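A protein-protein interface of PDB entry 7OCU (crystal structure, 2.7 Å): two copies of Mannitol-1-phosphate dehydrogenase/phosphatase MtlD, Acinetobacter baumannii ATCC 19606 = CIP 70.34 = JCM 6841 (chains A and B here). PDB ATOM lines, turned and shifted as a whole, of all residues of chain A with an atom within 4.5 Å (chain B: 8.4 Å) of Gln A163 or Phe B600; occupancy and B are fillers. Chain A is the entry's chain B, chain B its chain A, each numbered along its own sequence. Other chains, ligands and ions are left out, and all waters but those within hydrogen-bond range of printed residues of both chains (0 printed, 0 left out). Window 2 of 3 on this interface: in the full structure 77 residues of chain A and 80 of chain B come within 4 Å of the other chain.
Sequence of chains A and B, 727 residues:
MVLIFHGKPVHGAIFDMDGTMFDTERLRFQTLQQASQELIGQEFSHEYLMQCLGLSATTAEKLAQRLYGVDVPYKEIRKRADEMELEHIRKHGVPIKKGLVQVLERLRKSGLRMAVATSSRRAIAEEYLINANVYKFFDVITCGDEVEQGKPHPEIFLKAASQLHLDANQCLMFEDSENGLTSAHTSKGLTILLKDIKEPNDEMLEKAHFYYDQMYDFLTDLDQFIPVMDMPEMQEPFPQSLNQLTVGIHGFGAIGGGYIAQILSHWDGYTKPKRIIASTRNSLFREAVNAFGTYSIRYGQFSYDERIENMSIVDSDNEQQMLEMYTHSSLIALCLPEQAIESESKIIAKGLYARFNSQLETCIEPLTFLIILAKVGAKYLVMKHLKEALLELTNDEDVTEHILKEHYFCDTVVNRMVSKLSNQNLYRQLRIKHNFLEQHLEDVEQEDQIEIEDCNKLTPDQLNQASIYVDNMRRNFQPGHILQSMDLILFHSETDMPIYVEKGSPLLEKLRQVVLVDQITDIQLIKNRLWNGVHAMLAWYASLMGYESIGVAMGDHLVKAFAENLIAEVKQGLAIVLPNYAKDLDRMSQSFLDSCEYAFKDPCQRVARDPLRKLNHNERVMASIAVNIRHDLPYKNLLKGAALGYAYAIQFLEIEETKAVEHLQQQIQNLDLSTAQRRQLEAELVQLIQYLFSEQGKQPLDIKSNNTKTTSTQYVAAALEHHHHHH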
ATOM      1  N   VAL A 140      26.852 -24.180   2.606  1.00  0.00           N
ATOM      2  CA  VAL A 140      25.736 -23.368   2.033  1.00  0.00           C
ATOM      3  C   VAL A 140      26.060 -23.071   0.564  1.00  0.00           C
ATOM      4  O   VAL A 140      27.243 -23.166   0.192  1.00  0.00           O
ATOM      5  CB  VAL A 140      25.524 -22.061   2.823  1.00  0.00           C
ATOM      6  CG1 VAL A 140      24.127 -21.495   2.604  1.00  0.00           C
ATOM      7  CG2 VAL A 140      25.804 -22.238   4.309  1.00  0.00           C
ATOM      8  N   ILE A 141      25.043 -22.736  -0.236  1.00  0.00           N
ATOM      9  CA  ILE A 141      25.207 -22.199  -1.622  1.00  0.00           C
ATOM     10  C   ILE A 141      24.291 -20.980  -1.785  1.00  0.00           C
ATOM     11  O   ILE A 141      23.181 -20.988  -1.214  1.00  0.00           O
ATOM     12  CB  ILE A 141      24.946 -23.283  -2.690  1.00  0.00           C
ATOM     13  CG1 ILE A 141      23.488 -23.751  -2.724  1.00  0.00           C
ATOM     14  CG2 ILE A 141      25.903 -24.452  -2.506  1.00  0.00           C
ATOM     15  CD1 ILE A 141      23.112 -24.492  -3.987  1.00  0.00           C
ATOM     16  N   THR A 142      24.763 -19.968  -2.518  1.00  0.00           N
ATOM     17  CA  THR A 142      24.020 -18.723  -2.852  1.00  0.00           C
ATOM     18  C   THR A 142      23.870 -18.641  -4.373  1.00  0.00           C
ATOM     19  O   THR A 142      24.877 -18.856  -5.076  1.00  0.00           O
ATOM     20  CB  THR A 142      24.719 -17.485  -2.277  1.00  0.00           C
ATOM     21  OG1 THR A 142      25.145 -17.785  -0.945  1.00  0.00           O
ATOM     22  CG2 THR A 142      23.827 -16.264  -2.258  1.00  0.00           C
ATOM     23  N   LYS A 159      25.992 -12.352   1.397  1.00  0.00           N
ATOM     24  CA  LYS A 159      24.963 -13.334   1.838  1.00  0.00           C
ATOM     25  C   LYS A 159      25.627 -14.694   2.087  1.00  0.00           C
ATOM     26  O   LYS A 159      25.299 -15.332   3.107  1.00  0.00           O
ATOM     27  CB  LYS A 159      23.853 -13.449   0.787  1.00  0.00           C
ATOM     28  CG  LYS A 159      22.633 -14.261   1.204  1.00  0.00           C
ATOM     29  CD  LYS A 159      21.485 -14.163   0.219  1.00  0.00           C
ATOM     30  CE  LYS A 159      20.204 -14.792   0.726  1.00  0.00           C
ATOM     31  NZ  LYS A 159      20.352 -16.252   0.932  1.00  0.00           N
ATOM     32  N   ALA A 160      26.524 -15.111   1.187  1.00  0.00           N
ATOM     33  CA  ALA A 160      27.292 -16.377   1.261  1.00  0.00           C
ATOM     34  C   ALA A 160      28.148 -16.393   2.533  1.00  0.00           C
ATOM     35  O   ALA A 160      28.137 -17.421   3.236  1.00  0.00           O
ATOM     36  CB  ALA A 160      28.143 -16.538   0.025  1.00  0.00           C
ATOM     37  N   ALA A 161      28.852 -15.290   2.814  1.00  0.00           N
ATOM     38  CA  ALA A 161      29.754 -15.118   3.977  1.00  0.00           C
ATOM     39  C   ALA A 161      28.945 -15.130   5.281  1.00  0.00           C
ATOM     40  O   ALA A 161      29.395 -15.775   6.249  1.00  0.00           O
ATOM     41  CB  ALA A 161      30.542 -13.838   3.835  1.00  0.00           C
ATOM     42  N   SER A 162      27.800 -14.438   5.299  1.00  0.00           N
ATOM     43  CA  SER A 162      26.906 -14.289   6.478  1.00  0.00           C
ATOM     44  C   SER A 162      26.300 -15.644   6.864  1.00  0.00           C
ATOM     45  O   SER A 162      26.220 -15.927   8.076  1.00  0.00           O
ATOM     46  CB  SER A 162      25.832 -13.265   6.217  1.00  0.00           C
ATOM     47  OG  SER A 162      25.111 -12.974   7.404  1.00  0.00           O
ATOM     48  N   GLN A 163      25.896 -16.449   5.873  1.00  0.00           N
ATOM     49  CA  GLN A 163      25.255 -17.780   6.071  1.00  0.00           C
ATOM     50  C   GLN A 163      26.290 -18.796   6.576  1.00  0.00           C
ATOM     51  O   GLN A 163      25.877 -19.748   7.267  1.00  0.00           O
ATOM     52  CB  GLN A 163      24.602 -18.266   4.776  1.00  0.00           C
ATOM     53  CG  GLN A 163      23.268 -17.594   4.483  1.00  0.00           C
ATOM     54  CD  GLN A 163      22.605 -18.150   3.246  1.00  0.00           C
ATOM     55  OE1 GLN A 163      23.247 -18.385   2.224  1.00  0.00           O
ATOM     56  NE2 GLN A 163      21.302 -18.362   3.330  1.00  0.00           N
ATOM     57  N   LEU A 164      27.572 -18.607   6.242  1.00  0.00           N
ATOM     58  CA  LEU A 164      28.704 -19.436   6.742  1.00  0.00           C
ATOM     59  C   LEU A 164      29.044 -19.041   8.187  1.00  0.00           C
ATOM     60  O   LEU A 164      29.820 -19.781   8.825  1.00  0.00           O
ATOM     61  CB  LEU A 164      29.922 -19.253   5.830  1.00  0.00           C
ATOM     62  CG  LEU A 164      29.885 -20.014   4.504  1.00  0.00           C
ATOM     63  CD1 LEU A 164      31.015 -19.554   3.592  1.00  0.00           C
ATOM     64  CD2 LEU A 164      29.962 -21.517   4.736  1.00  0.00           C
ATOM     65  N   HIS A 165      28.496 -17.919   8.670  1.00  0.00           N
ATOM     66  CA  HIS A 165      28.688 -17.371  10.042  1.00  0.00           C
ATOM     67  C   HIS A 165      30.129 -16.868  10.183  1.00  0.00           C
ATOM     68  O   HIS A 165      30.793 -17.222  11.179  1.00  0.00           O
ATOM     69  CB  HIS A 165      28.296 -18.412  11.103  1.00  0.00           C
ATOM     70  CG  HIS A 165      27.013 -19.113  10.808  1.00  0.00           C
ATOM     71  ND1 HIS A 165      25.873 -18.435  10.423  1.00  0.00           N
ATOM     72  CD2 HIS A 165      26.683 -20.423  10.834  1.00  0.00           C
ATOM     73  CE1 HIS A 165      24.896 -19.295  10.228  1.00  0.00           C
ATOM     74  NE2 HIS A 165      25.367 -20.522  10.473  1.00  0.00           N
ATOM     75  N   SER B 419      18.618 -35.871   9.049  1.00  0.00           N
ATOM     76  CA  SER B 419      17.631 -35.313   8.087  1.00  0.00           C
ATOM     77  C   SER B 419      17.416 -36.310   6.942  1.00  0.00           C
ATOM     78  O   SER B 419      18.400 -36.624   6.241  1.00  0.00           O
ATOM     79  CB  SER B 419      18.086 -33.971   7.571  1.00  0.00           C
ATOM     80  OG  SER B 419      17.114 -33.401   6.708  1.00  0.00           O
ATOM     81  N   GLU B 494      24.785 -35.860  11.728  1.00  0.00           N
ATOM     82  CA  GLU B 494      25.892 -35.222  12.490  1.00  0.00           C
ATOM     83  C   GLU B 494      26.885 -36.307  12.927  1.00  0.00           C
ATOM     84  O   GLU B 494      26.657 -37.486  12.589  1.00  0.00           O
ATOM     85  CB  GLU B 494      25.325 -34.444  13.681  1.00  0.00           C
ATOM     86  CG  GLU B 494      24.374 -33.329  13.276  1.00  0.00           C
ATOM     87  CD  GLU B 494      24.990 -32.259  12.391  1.00  0.00           C
ATOM     88  OE1 GLU B 494      24.273 -31.736  11.516  1.00  0.00           O
ATOM     89  OE2 GLU B 494      26.185 -31.951  12.576  1.00  0.00           O
ATOM     90  N   GLU B 548      14.115 -17.974  11.444  1.00  0.00           N
ATOM     91  CA  GLU B 548      13.247 -19.135  11.100  1.00  0.00           C
ATOM     92  C   GLU B 548      13.882 -20.420  11.646  1.00  0.00           C
ATOM     93  O   GLU B 548      13.214 -21.114  12.438  1.00  0.00           O
ATOM     94  CB  GLU B 548      13.047 -19.231   9.586  1.00  0.00           C
ATOM     95  CG  GLU B 548      12.376 -18.010   8.973  1.00  0.00           C
ATOM     96  CD  GLU B 548      10.917 -17.798   9.348  1.00  0.00           C
ATOM     97  OE1 GLU B 548      10.292 -18.740   9.876  1.00  0.00           O
ATOM     98  OE2 GLU B 548      10.408 -16.687   9.106  1.00  0.00           O
ATOM     99  N   SER B 549      15.117 -20.716  11.229  1.00  0.00           N
ATOM    100  CA  SER B 549      15.914 -21.898  11.655  1.00  0.00           C
ATOM    101  C   SER B 549      16.976 -21.471  12.674  1.00  0.00           C
ATOM    102  O   SER B 549      17.406 -20.301  12.631  1.00  0.00           O
ATOM    103  CB  SER B 549      16.540 -22.587  10.468  1.00  0.00           C
ATOM    104  OG  SER B 549      17.509 -21.754   9.849  1.00  0.00           O
ATOM    105  N   ILE B 550      17.388 -22.398  13.545  1.00  0.00           N
ATOM    106  CA  ILE B 550      18.402 -22.162  14.617  1.00  0.00           C
ATOM    107  C   ILE B 550      19.793 -22.072  13.972  1.00  0.00           C
ATOM    108  O   ILE B 550      20.682 -21.456  14.588  1.00  0.00           O
ATOM    109  CB  ILE B 550      18.319 -23.255  15.706  1.00  0.00           C
ATOM    110  CG1 ILE B 550      18.565 -22.686  17.107  1.00  0.00           C
ATOM    111  CG2 ILE B 550      19.247 -24.423  15.403  1.00  0.00           C
ATOM    112  CD1 ILE B 550      18.086 -23.586  18.223  1.00  0.00           C
ATOM    113  N   GLY B 551      19.964 -22.670  12.786  1.00  0.00           N
ATOM    114  CA  GLY B 551      21.206 -22.623  11.988  1.00  0.00           C
ATOM    115  C   GLY B 551      21.557 -21.206  11.566  1.00  0.00           C
ATOM    116  O   GLY B 551      22.708 -20.793  11.805  1.00  0.00           O
ATOM    117  N   VAL B 552      20.600 -20.489  10.963  1.00  0.00           N
ATOM    118  CA  VAL B 552      20.749 -19.072  10.508  1.00  0.00           C
ATOM    119  C   VAL B 552      21.025 -18.189  11.732  1.00  0.00           C
ATOM    120  O   VAL B 552      21.844 -17.256  11.609  1.00  0.00           O
ATOM    121  CB  VAL B 552      19.506 -18.589   9.731  1.00  0.00           C
ATOM    122  CG1 VAL B 552      19.530 -17.085   9.488  1.00  0.00           C
ATOM    123  CG2 VAL B 552      19.337 -19.333   8.416  1.00  0.00           C
ATOM    124  N   ALA B 553      20.371 -18.483  12.861  1.00  0.00           N
ATOM    125  CA  ALA B 553      20.425 -17.702  14.120  1.00  0.00           C
ATOM    126  C   ALA B 553      21.855 -17.663  14.676  1.00  0.00           C
ATOM    127  O   ALA B 553      22.224 -16.624  15.258  1.00  0.00           O
ATOM    128  CB  ALA B 553      19.461 -18.280  15.129  1.00  0.00           C
ATOM    129  N   MET B 554      22.628 -18.742  14.498  1.00  0.00           N
ATOM    130  CA  MET B 554      24.023 -18.875  15.009  1.00  0.00           C
ATOM    131  C   MET B 554      24.946 -17.863  14.314  1.00  0.00           C
ATOM    132  O   MET B 554      26.018 -17.572  14.881  1.00  0.00           O
ATOM    133  CB  MET B 554      24.563 -20.293  14.787  1.00  0.00           C
ATOM    134  CG  MET B 554      23.866 -21.350  15.629  1.00  0.00           C
ATOM    135  SD  MET B 554      24.234 -21.229  17.402  1.00  0.00           S
ATOM    136  CE  MET B 554      25.900 -21.887  17.440  1.00  0.00           C
ATOM    137  N   GLY B 555      24.555 -17.359  13.137  1.00  0.00           N
ATOM    138  CA  GLY B 555      25.245 -16.264  12.424  1.00  0.00           C
ATOM    139  C   GLY B 555      25.302 -14.992  13.255  1.00  0.00           C
ATOM    140  O   GLY B 555      26.318 -14.275  13.164  1.00  0.00           O
ATOM    141  N   SER B 595      26.375 -29.325  15.893  1.00  0.00           N
ATOM    142  CA  SER B 595      25.119 -29.682  15.180  1.00  0.00           C
ATOM    143  C   SER B 595      24.244 -28.437  14.978  1.00  0.00           C
ATOM    144  O   SER B 595      23.569 -28.363  13.933  1.00  0.00           O
ATOM    145  CB  SER B 595      24.371 -30.767  15.913  1.00  0.00           C
ATOM    146  OG  SER B 595      24.120 -30.390  17.258  1.00  0.00           O
ATOM    147  N   CYS B 596      24.259 -27.504  15.936  1.00  0.00           N
ATOM    148  CA  CYS B 596      23.468 -26.241  15.925  1.00  0.00           C
ATOM    149  C   CYS B 596      23.941 -25.302  14.807  1.00  0.00           C
ATOM    150  O   CYS B 596      23.099 -24.531  14.305  1.00  0.00           O
ATOM    151  CB  CYS B 596      23.573 -25.505  17.258  1.00  0.00           C
ATOM    152  SG  CYS B 596      22.592 -26.255  18.582  1.00  0.00           S
ATOM    153  N   GLU B 597      25.228 -25.358  14.447  1.00  0.00           N
ATOM    154  CA  GLU B 597      25.910 -24.363  13.572  1.00  0.00           C
ATOM    155  C   GLU B 597      25.163 -24.230  12.239  1.00  0.00           C
ATOM    156  O   GLU B 597      24.725 -23.106  11.928  1.00  0.00           O
ATOM    157  CB  GLU B 597      27.374 -24.751  13.349  1.00  0.00           C
ATOM    158  CG  GLU B 597      28.241 -23.601  12.863  1.00  0.00           C
ATOM    159  CD  GLU B 597      28.359 -22.428  13.823  1.00  0.00           C
ATOM    160  OE1 GLU B 597      28.562 -21.293  13.345  1.00  0.00           O
ATOM    161  OE2 GLU B 597      28.249 -22.648  15.045  1.00  0.00           O
ATOM    162  N   TYR B 598      25.022 -25.329  11.490  1.00  0.00           N
ATOM    163  CA  TYR B 598      24.387 -25.365  10.144  1.00  0.00           C
ATOM    164  C   TYR B 598      23.102 -26.202  10.191  1.00  0.00           C
ATOM    165  O   TYR B 598      22.889 -27.034   9.286  1.00  0.00           O
ATOM    166  CB  TYR B 598      25.379 -25.890   9.103  1.00  0.00           C
ATOM    167  CG  TYR B 598      26.584 -25.009   8.886  1.00  0.00           C
ATOM    168  CD1 TYR B 598      26.437 -23.661   8.603  1.00  0.00           C
ATOM    169  CD2 TYR B 598      27.870 -25.521   8.948  1.00  0.00           C
ATOM    170  CE1 TYR B 598      27.534 -22.839   8.399  1.00  0.00           C
ATOM    171  CE2 TYR B 598      28.978 -24.714   8.743  1.00  0.00           C
ATOM    172  CZ  TYR B 598      28.809 -23.369   8.466  1.00  0.00           C
ATOM    173  OH  TYR B 598      29.893 -22.563   8.266  1.00  0.00           O
ATOM    174  N   ALA B 599      22.262 -25.964  11.205  1.00  0.00           N
ATOM    175  CA  ALA B 599      20.942 -26.612  11.394  1.00  0.00           C
ATOM    176  C   ALA B 599      19.862 -25.761  10.713  1.00  0.00           C
ATOM    177  O   ALA B 599      18.968 -25.250  11.417  1.00  0.00           O
ATOM    178  CB  ALA B 599      20.664 -26.804  12.865  1.00  0.00           C
ATOM    179  N   PHE B 600      19.957 -25.621   9.386  1.00  0.00           N
ATOM    180  CA  PHE B 600      19.026 -24.829   8.537  1.00  0.00           C
ATOM    181  C   PHE B 600      17.705 -25.588   8.368  1.00  0.00           C
ATOM    182  O   PHE B 600      16.665 -24.936   8.149  1.00  0.00           O
ATOM    183  CB  PHE B 600      19.652 -24.539   7.170  1.00  0.00           C
ATOM    184  CG  PHE B 600      20.966 -23.801   7.216  1.00  0.00           C
ATOM    185  CD1 PHE B 600      21.050 -22.543   7.793  1.00  0.00           C
ATOM    186  CD2 PHE B 600      22.116 -24.357   6.676  1.00  0.00           C
ATOM    187  CE1 PHE B 600      22.255 -21.859   7.834  1.00  0.00           C
ATOM    188  CE2 PHE B 600      23.322 -23.672   6.717  1.00  0.00           C
ATOM    189  CZ  PHE B 600      23.388 -22.425   7.294  1.00  0.00           C
ATOM    190  N   LYS B 601      17.755 -26.920   8.471  1.00  0.00           N
ATOM    191  CA  LYS B 601      16.607 -27.837   8.232  1.00  0.00           C
ATOM    192  C   LYS B 601      15.834 -28.064   9.541  1.00  0.00           C
ATOM    193  O   LYS B 601      14.782 -28.732   9.484  1.00  0.00           O
ATOM    194  CB  LYS B 601      17.107 -29.163   7.644  1.00  0.00           C
ATOM    195  CG  LYS B 601      16.397 -29.617   6.375  1.00  0.00           C
ATOM    196  CD  LYS B 601      16.731 -28.769   5.162  1.00  0.00           C
ATOM    197  CE  LYS B 601      15.927 -29.136   3.932  1.00  0.00           C
ATOM    198  NZ  LYS B 601      16.295 -30.474   3.411  1.00  0.00           N
ATOM    199  N   ASP B 602      16.335 -27.535  10.665  1.00  0.00           N
ATOM    200  CA  ASP B 602      15.722 -27.660  12.016  1.00  0.00           C
ATOM    201  C   ASP B 602      14.945 -26.384  12.334  1.00  0.00           C
ATOM    202  O   ASP B 602      15.547 -25.358  12.648  1.00  0.00           O
ATOM    203  CB  ASP B 602      16.791 -27.935  13.078  1.00  0.00           C
ATOM    204  CG  ASP B 602      16.236 -28.149  14.477  1.00  0.00           C
ATOM    205  OD1 ASP B 602      16.819 -27.592  15.429  1.00  0.00           O
ATOM    206  OD2 ASP B 602      15.229 -28.876  14.605  1.00  0.00           O
ATOM    207  N   PRO B 603      13.591 -26.401  12.270  1.00  0.00           N
ATOM    208  CA  PRO B 603      12.791 -25.205  12.539  1.00  0.00           C
ATOM    209  C   PRO B 603      12.708 -24.879  14.039  1.00  0.00           C
ATOM    210  O   PRO B 603      12.686 -25.797  14.839  1.00  0.00           O
ATOM    211  CB  PRO B 603      11.412 -25.572  11.971  1.00  0.00           C
ATOM    212  CG  PRO B 603      11.335 -27.076  12.136  1.00  0.00           C
ATOM    213  CD  PRO B 603      12.755 -27.568  11.943  1.00  0.00           C
ATOM    214  N   CYS B 604      12.664 -23.584  14.372  1.00  0.00           N
ATOM    215  CA  CYS B 604      12.625 -23.051  15.761  1.00  0.00           C
ATOM    216  C   CYS B 604      11.275 -23.366  16.418  1.00  0.00           C
ATOM    217  O   CYS B 604      11.256 -23.559  17.650  1.00  0.00           O
ATOM    218  CB  CYS B 604      12.871 -21.547  15.780  1.00  0.00           C
ATOM    219  SG  CYS B 604      14.510 -21.078  15.166  1.00  0.00           S
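Printed residues of chain B within 4 Å of Val A140: Phe B600. No residue of chain B comes within 4 Å of Ser A162. Gln A163 touches just these residues of chain B: Tyr B598 (3.7 Å) and Phe B600 (3.7 Å). Printed residues of chain B within 4 Å of Leu A164: Tyr B598 (2.8 Å). Of the printed residues of chain A, Val B552 touches His A165 (3.9 Å). Cys B596 touches none of the printed residues of chain A. Of the printed residues of chain A, Tyr B598 touches Gln A163 (3.7 Å), Leu A164 (2.8 Å) and His A165 (3.5 Å). Phe B600 touches two residues of chain A.
Among the printed residues, pairs that only touch across the chains: Val A140 with Phe B600 (3.7 Å), Gln A163 with Tyr B598 (3.7 Å), Gln A163 with Phe B600 (3.7 Å), His A165 with Val B552 (3.9 Å) and His A165 with Tyr B598 (3.5 Å).
The side-chain amide nitrogen of Gln A163 sits close to the side-chain amino group of Lys A159, at 3.3 Å. The backbone NH of Gly B551 sits at hydrogen-bond distance from the backbone carbonyl oxygen of Ala B599 (3.1 Å). ND1 of His A165 lies within hydrogen-bond range of O of Ser A162. The backbone carbonyl oxygen (O) of Gln A163 lies close to a ring nitrogen (NE2) of His A165.
A ring nitrogen (NE2) of His A165 is in hydrogen-bond range of the backbone carbonyl oxygen (O) of Gly B551, at 3.0 Å. NE2 of His A165 sits at hydrogen-bond distance from O of Glu B597, 3.0 Å away. N of Gly B555 lies close to ND1 of His A165. The side-chain hydroxyl of Tyr B598 lies within hydrogen-bond range of the backbone carbonyl oxygen of Leu A164.
No position is printed for both chains.
Hydrophobic or aromatic side chains of chain B that line the printed part of chain A: Tyr B598 and Phe B600. Of the 10 printed residues of chain A, 4 touch a printed residue of chain B.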
